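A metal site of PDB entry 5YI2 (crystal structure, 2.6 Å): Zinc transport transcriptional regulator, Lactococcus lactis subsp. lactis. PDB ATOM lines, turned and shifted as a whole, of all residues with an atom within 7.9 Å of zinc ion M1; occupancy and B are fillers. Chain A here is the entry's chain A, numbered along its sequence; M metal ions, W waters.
The backbone NH (N) of Glu 31 sits at hydrogen-bond distance from the side-chain carboxylate (OE2) of Glu 107, 3.1 Å away. OE1 of Glu 107 sits close to OG of Ser 32, 3.0 Å away. The side-chain sulfur (SG) of Cys 30 lies close to the backbone NH (N) of Ser 32, 3.6 Å away. The side-chain carboxylate (OE1) of Glu 41 sits close to a ring nitrogen (ND1) of His 108, 3.3 Å away.
Ser 32 touches zinc ion M1. ND1 of His 108 touches zinc ion M1, 3.96 Å away. Five residues have an atom within 4 Å of zinc ion M1: Cys 30, Ser 32, Glu 41, Glu 107 and His 108. The nearest printed residue that does not touch zinc ion M1 is His 111 (4.04 Å).
Zinc ion M1 is bound by water W1 (2.1 Å), the side-chain carboxylate (OE1) of Glu 107 (2.1 Å), the side-chain carboxylate (OE1) of Glu 41 (2.2 Å) and the side-chain sulfur (SG) of Cys 30 (2.6 Å). Zinc ion M1 has four donor atoms within binding distance.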
ATOM      1  N   LEU A  26      -7.970 -28.833 -20.781  1.00  0.00           N
ATOM      2  CA  LEU A  26      -7.094 -28.531 -21.914  1.00  0.00           C
ATOM      3  C   LEU A  26      -5.709 -29.116 -21.695  1.00  0.00           C
ATOM      4  O   LEU A  26      -5.179 -29.066 -20.582  1.00  0.00           O
ATOM      5  CB  LEU A  26      -6.966 -27.016 -22.105  1.00  0.00           C
ATOM      6  CG  LEU A  26      -8.219 -26.229 -22.466  1.00  0.00           C
ATOM      7  CD1 LEU A  26      -7.973 -24.730 -22.311  1.00  0.00           C
ATOM      8  CD2 LEU A  26      -8.678 -26.581 -23.884  1.00  0.00           C
ATOM      9  N   LYS A  29       0.498 -26.436 -21.976  1.00  0.00           N
ATOM     10  CA  LYS A  29       0.549 -25.191 -21.226  1.00  0.00           C
ATOM     11  C   LYS A  29      -0.303 -24.095 -21.878  1.00  0.00           C
ATOM     12  O   LYS A  29      -0.453 -24.055 -23.100  1.00  0.00           O
ATOM     13  CB  LYS A  29       2.013 -24.736 -21.087  1.00  0.00           C
ATOM     14  CG  LYS A  29       2.235 -23.595 -20.098  1.00  0.00           C
ATOM     15  CD  LYS A  29       3.718 -23.229 -19.957  1.00  0.00           C
ATOM     16  CE  LYS A  29       3.900 -22.039 -18.999  1.00  0.00           C
ATOM     17  NZ  LYS A  29       5.332 -21.663 -18.788  1.00  0.00           N
ATOM     18  N   CYS A  30      -0.893 -23.233 -21.045  1.00  0.00           N
ATOM     19  CA  CYS A  30      -1.538 -22.031 -21.542  1.00  0.00           C
ATOM     20  C   CYS A  30      -0.480 -21.006 -21.940  1.00  0.00           C
ATOM     21  O   CYS A  30       0.099 -20.318 -21.089  1.00  0.00           O
ATOM     22  CB  CYS A  30      -2.468 -21.415 -20.505  1.00  0.00           C
ATOM     23  SG  CYS A  30      -2.990 -19.727 -20.901  1.00  0.00           S
ATOM     24  N   GLU A  31      -0.241 -20.916 -23.244  1.00  0.00           N
ATOM     25  CA  GLU A  31       0.810 -20.061 -23.782  1.00  0.00           C
ATOM     26  C   GLU A  31       0.430 -18.567 -23.859  1.00  0.00           C
ATOM     27  O   GLU A  31       1.063 -17.794 -24.577  1.00  0.00           O
ATOM     28  CB  GLU A  31       1.249 -20.572 -25.158  1.00  0.00           C
ATOM     29  CG  GLU A  31       1.838 -21.984 -25.131  1.00  0.00           C
ATOM     30  CD  GLU A  31       2.074 -22.551 -26.527  1.00  0.00           C
ATOM     31  OE1 GLU A  31       2.235 -23.786 -26.651  1.00  0.00           O
ATOM     32  OE2 GLU A  31       2.115 -21.768 -27.511  1.00  0.00           O
ATOM     33  N   SER A  32      -0.601 -18.157 -23.122  1.00  0.00           N
ATOM     34  CA  SER A  32      -0.954 -16.741 -23.076  1.00  0.00           C
ATOM     35  C   SER A  32      -0.074 -15.935 -22.116  1.00  0.00           C
ATOM     36  O   SER A  32       0.152 -16.357 -20.972  1.00  0.00           O
ATOM     37  CB  SER A  32      -2.439 -16.562 -22.715  1.00  0.00           C
ATOM     38  OG  SER A  32      -3.242 -16.511 -23.878  1.00  0.00           O
ATOM     39  N   ASP A  33       0.401 -14.783 -22.581  1.00  0.00           N
ATOM     40  CA  ASP A  33       1.237 -13.888 -21.781  1.00  0.00           C
ATOM     41  C   ASP A  33       0.524 -13.380 -20.533  1.00  0.00           C
ATOM     42  O   ASP A  33       1.171 -12.986 -19.570  1.00  0.00           O
ATOM     43  CB  ASP A  33       1.732 -12.725 -22.624  1.00  0.00           C
ATOM     44  N   VAL A  34      -0.813 -13.370 -20.552  1.00  0.00           N
ATOM     45  CA  VAL A  34      -1.552 -12.919 -19.374  1.00  0.00           C
ATOM     46  C   VAL A  34      -1.980 -14.089 -18.502  1.00  0.00           C
ATOM     47  O   VAL A  34      -2.282 -15.182 -19.018  1.00  0.00           O
ATOM     48  CB  VAL A  34      -2.799 -12.110 -19.745  1.00  0.00           C
ATOM     49  CG1 VAL A  34      -3.312 -11.382 -18.516  1.00  0.00           C
ATOM     50  CG2 VAL A  34      -2.472 -11.132 -20.856  1.00  0.00           C
ATOM     51  N   LEU A  36      -4.622 -15.826 -16.747  1.00  0.00           N
ATOM     52  CA  LEU A  36      -6.068 -15.898 -16.611  1.00  0.00           C
ATOM     53  C   LEU A  36      -6.539 -17.342 -16.420  1.00  0.00           C
ATOM     54  O   LEU A  36      -5.919 -18.287 -16.928  1.00  0.00           O
ATOM     55  CB  LEU A  36      -6.753 -15.288 -17.840  1.00  0.00           C
ATOM     56  CG  LEU A  36      -6.519 -13.805 -18.152  1.00  0.00           C
ATOM     57  CD1 LEU A  36      -7.087 -13.476 -19.520  1.00  0.00           C
ATOM     58  CD2 LEU A  36      -7.145 -12.933 -17.089  1.00  0.00           C
ATOM     59  N   THR A  37      -7.625 -17.500 -15.679  1.00  0.00           N
ATOM     60  CA  THR A  37      -8.276 -18.792 -15.570  1.00  0.00           C
ATOM     61  C   THR A  37      -8.765 -19.200 -16.956  1.00  0.00           C
ATOM     62  O   THR A  37      -8.967 -18.345 -17.824  1.00  0.00           O
ATOM     63  CB  THR A  37      -9.523 -18.714 -14.676  1.00  0.00           C
ATOM     64  OG1 THR A  37     -10.427 -17.762 -15.227  1.00  0.00           O
ATOM     65  CG2 THR A  37      -9.154 -18.298 -13.269  1.00  0.00           C
ATOM     66  N   SER A  38      -8.957 -20.499 -17.158  1.00  0.00           N
ATOM     67  CA  SER A  38      -9.466 -20.966 -18.453  1.00  0.00           C
ATOM     68  C   SER A  38     -10.870 -20.422 -18.692  1.00  0.00           C
ATOM     69  O   SER A  38     -11.234 -20.133 -19.832  1.00  0.00           O
ATOM     70  CB  SER A  38      -9.444 -22.487 -18.532  1.00  0.00           C
ATOM     71  OG  SER A  38     -10.286 -23.067 -17.544  1.00  0.00           O
ATOM     72  N   GLU A  41     -10.443 -16.794 -19.989  1.00  0.00           N
ATOM     73  CA  GLU A  41      -9.927 -16.817 -21.346  1.00  0.00           C
ATOM     74  C   GLU A  41     -11.003 -17.306 -22.315  1.00  0.00           C
ATOM     75  O   GLU A  41     -11.160 -16.792 -23.424  1.00  0.00           O
ATOM     76  CB  GLU A  41      -8.677 -17.691 -21.438  1.00  0.00           C
ATOM     77  CG  GLU A  41      -7.447 -17.094 -20.773  1.00  0.00           C
ATOM     78  CD  GLU A  41      -6.162 -17.690 -21.300  1.00  0.00           C
ATOM     79  OE1 GLU A  41      -6.220 -18.597 -22.139  1.00  0.00           O
ATOM     80  OE2 GLU A  41      -5.076 -17.249 -20.864  1.00  0.00           O
ATOM     81  N   HIS A  42     -11.752 -18.299 -21.876  1.00  0.00           N
ATOM     82  CA  HIS A  42     -12.809 -18.848 -22.708  1.00  0.00           C
ATOM     83  C   HIS A  42     -13.898 -17.813 -22.969  1.00  0.00           C
ATOM     84  O   HIS A  42     -14.510 -17.783 -24.033  1.00  0.00           O
ATOM     85  CB  HIS A  42     -13.388 -20.113 -22.071  1.00  0.00           C
ATOM     86  CG  HIS A  42     -14.211 -20.937 -23.001  1.00  0.00           C
ATOM     87  ND1 HIS A  42     -13.773 -22.128 -23.525  1.00  0.00           N
ATOM     88  CD2 HIS A  42     -15.445 -20.729 -23.523  1.00  0.00           C
ATOM     89  CE1 HIS A  42     -14.698 -22.627 -24.326  1.00  0.00           C
ATOM     90  NE2 HIS A  42     -15.727 -21.798 -24.335  1.00  0.00           N
ATOM     91  N   PRO A 103      -5.450 -11.152 -29.115  1.00  0.00           N
ATOM     92  CA  PRO A 103      -4.478 -12.272 -29.186  1.00  0.00           C
ATOM     93  C   PRO A 103      -4.710 -13.350 -28.117  1.00  0.00           C
ATOM     94  O   PRO A 103      -4.615 -14.536 -28.431  1.00  0.00           O
ATOM     95  CB  PRO A 103      -3.126 -11.571 -28.961  1.00  0.00           C
ATOM     96  CG  PRO A 103      -3.460 -10.272 -28.296  1.00  0.00           C
ATOM     97  CD  PRO A 103      -4.788  -9.859 -28.840  1.00  0.00           C
ATOM     98  N   VAL A 104      -5.007 -12.957 -26.885  1.00  0.00           N
ATOM     99  CA  VAL A 104      -5.314 -13.909 -25.826  1.00  0.00           C
ATOM    100  C   VAL A 104      -6.487 -14.772 -26.233  1.00  0.00           C
ATOM    101  O   VAL A 104      -6.497 -15.978 -26.012  1.00  0.00           O
ATOM    102  CB  VAL A 104      -5.657 -13.205 -24.496  1.00  0.00           C
ATOM    103  CG1 VAL A 104      -6.026 -14.244 -23.433  1.00  0.00           C
ATOM    104  CG2 VAL A 104      -4.501 -12.340 -24.005  1.00  0.00           C
ATOM    105  N   ALA A 105      -7.488 -14.147 -26.829  1.00  0.00           N
ATOM    106  CA  ALA A 105      -8.656 -14.863 -27.308  1.00  0.00           C
ATOM    107  C   ALA A 105      -8.256 -15.896 -28.354  1.00  0.00           C
ATOM    108  O   ALA A 105      -8.711 -17.044 -28.330  1.00  0.00           O
ATOM    109  CB  ALA A 105      -9.678 -13.888 -27.889  1.00  0.00           C
ATOM    110  N   LYS A 106      -7.410 -15.462 -29.281  1.00  0.00           N
ATOM    111  CA  LYS A 106      -6.878 -16.302 -30.337  1.00  0.00           C
ATOM    112  C   LYS A 106      -6.072 -17.475 -29.763  1.00  0.00           C
ATOM    113  O   LYS A 106      -6.234 -18.614 -30.193  1.00  0.00           O
ATOM    114  CB  LYS A 106      -6.021 -15.463 -31.271  1.00  0.00           C
ATOM    115  CG  LYS A 106      -5.282 -16.255 -32.338  1.00  0.00           C
ATOM    116  CD  LYS A 106      -6.235 -16.696 -33.405  1.00  0.00           C
ATOM    117  CE  LYS A 106      -5.551 -17.630 -34.390  1.00  0.00           C
ATOM    118  NZ  LYS A 106      -6.521 -18.074 -35.434  1.00  0.00           N
ATOM    119  N   GLU A 107      -5.207 -17.206 -28.783  1.00  0.00           N
ATOM    120  CA  GLU A 107      -4.405 -18.253 -28.160  1.00  0.00           C
ATOM    121  C   GLU A 107      -5.309 -19.314 -27.527  1.00  0.00           C
ATOM    122  O   GLU A 107      -5.093 -20.499 -27.719  1.00  0.00           O
ATOM    123  CB  GLU A 107      -3.431 -17.675 -27.139  1.00  0.00           C
ATOM    124  CG  GLU A 107      -2.457 -18.689 -26.502  1.00  0.00           C
ATOM    125  CD  GLU A 107      -3.117 -19.599 -25.463  1.00  0.00           C
ATOM    126  OE1 GLU A 107      -4.144 -19.186 -24.890  1.00  0.00           O
ATOM    127  OE2 GLU A 107      -2.614 -20.723 -25.222  1.00  0.00           O
ATOM    128  N   HIS A 108      -6.318 -18.883 -26.773  1.00  0.00           N
ATOM    129  CA  HIS A 108      -7.247 -19.824 -26.158  1.00  0.00           C
ATOM    130  C   HIS A 108      -7.928 -20.718 -27.197  1.00  0.00           C
ATOM    131  O   HIS A 108      -8.034 -21.930 -27.002  1.00  0.00           O
ATOM    132  CB  HIS A 108      -8.275 -19.103 -25.281  1.00  0.00           C
ATOM    133  CG  HIS A 108      -9.034 -20.023 -24.358  1.00  0.00           C
ATOM    134  ND1 HIS A 108      -8.426 -20.753 -23.358  1.00  0.00           N
ATOM    135  CD2 HIS A 108     -10.356 -20.331 -24.288  1.00  0.00           C
ATOM    136  CE1 HIS A 108      -9.331 -21.463 -22.712  1.00  0.00           C
ATOM    137  NE2 HIS A 108     -10.512 -21.218 -23.262  1.00  0.00           N
ATOM    138  N   ALA A 109      -8.396 -20.149 -28.303  1.00  0.00           N
ATOM    139  CA  ALA A 109      -8.989 -20.953 -29.371  1.00  0.00           C
ATOM    140  C   ALA A 109      -8.009 -21.996 -29.915  1.00  0.00           C
ATOM    141  O   ALA A 109      -8.396 -23.118 -30.276  1.00  0.00           O
ATOM    142  CB  ALA A 109      -9.489 -20.083 -30.503  1.00  0.00           C
ATOM    143  N   THR A 110      -6.741 -21.603 -29.960  1.00  0.00           N
ATOM    144  CA  THR A 110      -5.697 -22.450 -30.493  1.00  0.00           C
ATOM    145  C   THR A 110      -5.439 -23.600 -29.521  1.00  0.00           C
ATOM    146  O   THR A 110      -5.360 -24.771 -29.923  1.00  0.00           O
ATOM    147  CB  THR A 110      -4.422 -21.630 -30.736  1.00  0.00           C
ATOM    148  OG1 THR A 110      -4.748 -20.462 -31.492  1.00  0.00           O
ATOM    149  CG2 THR A 110      -3.391 -22.439 -31.518  1.00  0.00           C
ATOM    150  N   HIS A 111      -5.347 -23.268 -28.246  1.00  0.00           N
ATOM    151  CA  HIS A 111      -5.185 -24.250 -27.197  1.00  0.00           C
ATOM    152  C   HIS A 111      -6.237 -25.347 -27.313  1.00  0.00           C
ATOM    153  O   HIS A 111      -5.917 -26.534 -27.238  1.00  0.00           O
ATOM    154  CB  HIS A 111      -5.284 -23.579 -25.828  1.00  0.00           C
ATOM    155  CG  HIS A 111      -4.636 -24.353 -24.735  1.00  0.00           C
ATOM    156  ND1 HIS A 111      -4.347 -23.809 -23.500  1.00  0.00           N
ATOM    157  CD2 HIS A 111      -4.208 -25.639 -24.684  1.00  0.00           C
ATOM    158  CE1 HIS A 111      -3.770 -24.715 -22.739  1.00  0.00           C
ATOM    159  NE2 HIS A 111      -3.682 -25.842 -23.434  1.00  0.00           N
ATOM    160  N   HIS A 112      -7.487 -24.945 -27.505  1.00  0.00           N
ATOM    161  CA  HIS A 112      -8.570 -25.905 -27.730  1.00  0.00           C
ATOM    162  C   HIS A 112      -8.324 -26.744 -28.982  1.00  0.00           C
ATOM    163  O   HIS A 112      -8.561 -27.953 -28.967  1.00  0.00           O
ATOM    164  CB  HIS A 112      -9.906 -25.181 -27.878  1.00  0.00           C
ATOM    165  CG  HIS A 112     -10.641 -25.000 -26.585  1.00  0.00           C
ATOM    166  ND1 HIS A 112     -11.468 -25.966 -26.050  1.00  0.00           N
ATOM    167  CD2 HIS A 112     -10.708 -23.943 -25.736  1.00  0.00           C
ATOM    168  CE1 HIS A 112     -12.002 -25.524 -24.928  1.00  0.00           C
ATOM    169  NE2 HIS A 112     -11.557 -24.295 -24.712  1.00  0.00           N
HETATM  170 ZN    ZN M   1      -4.600 -19.819 -22.923  1.00  0.00          ZN
HETATM  171 ZN    ZN M   2     -11.831 -22.896 -23.176  1.00  0.00          ZN
HETATM  172  O   HOH W   1      -5.297 -21.788 -22.686  1.00  0.00           O
HETATM  173  O   HOH W   2      -6.411 -21.553 -20.555  1.00  0.00           O
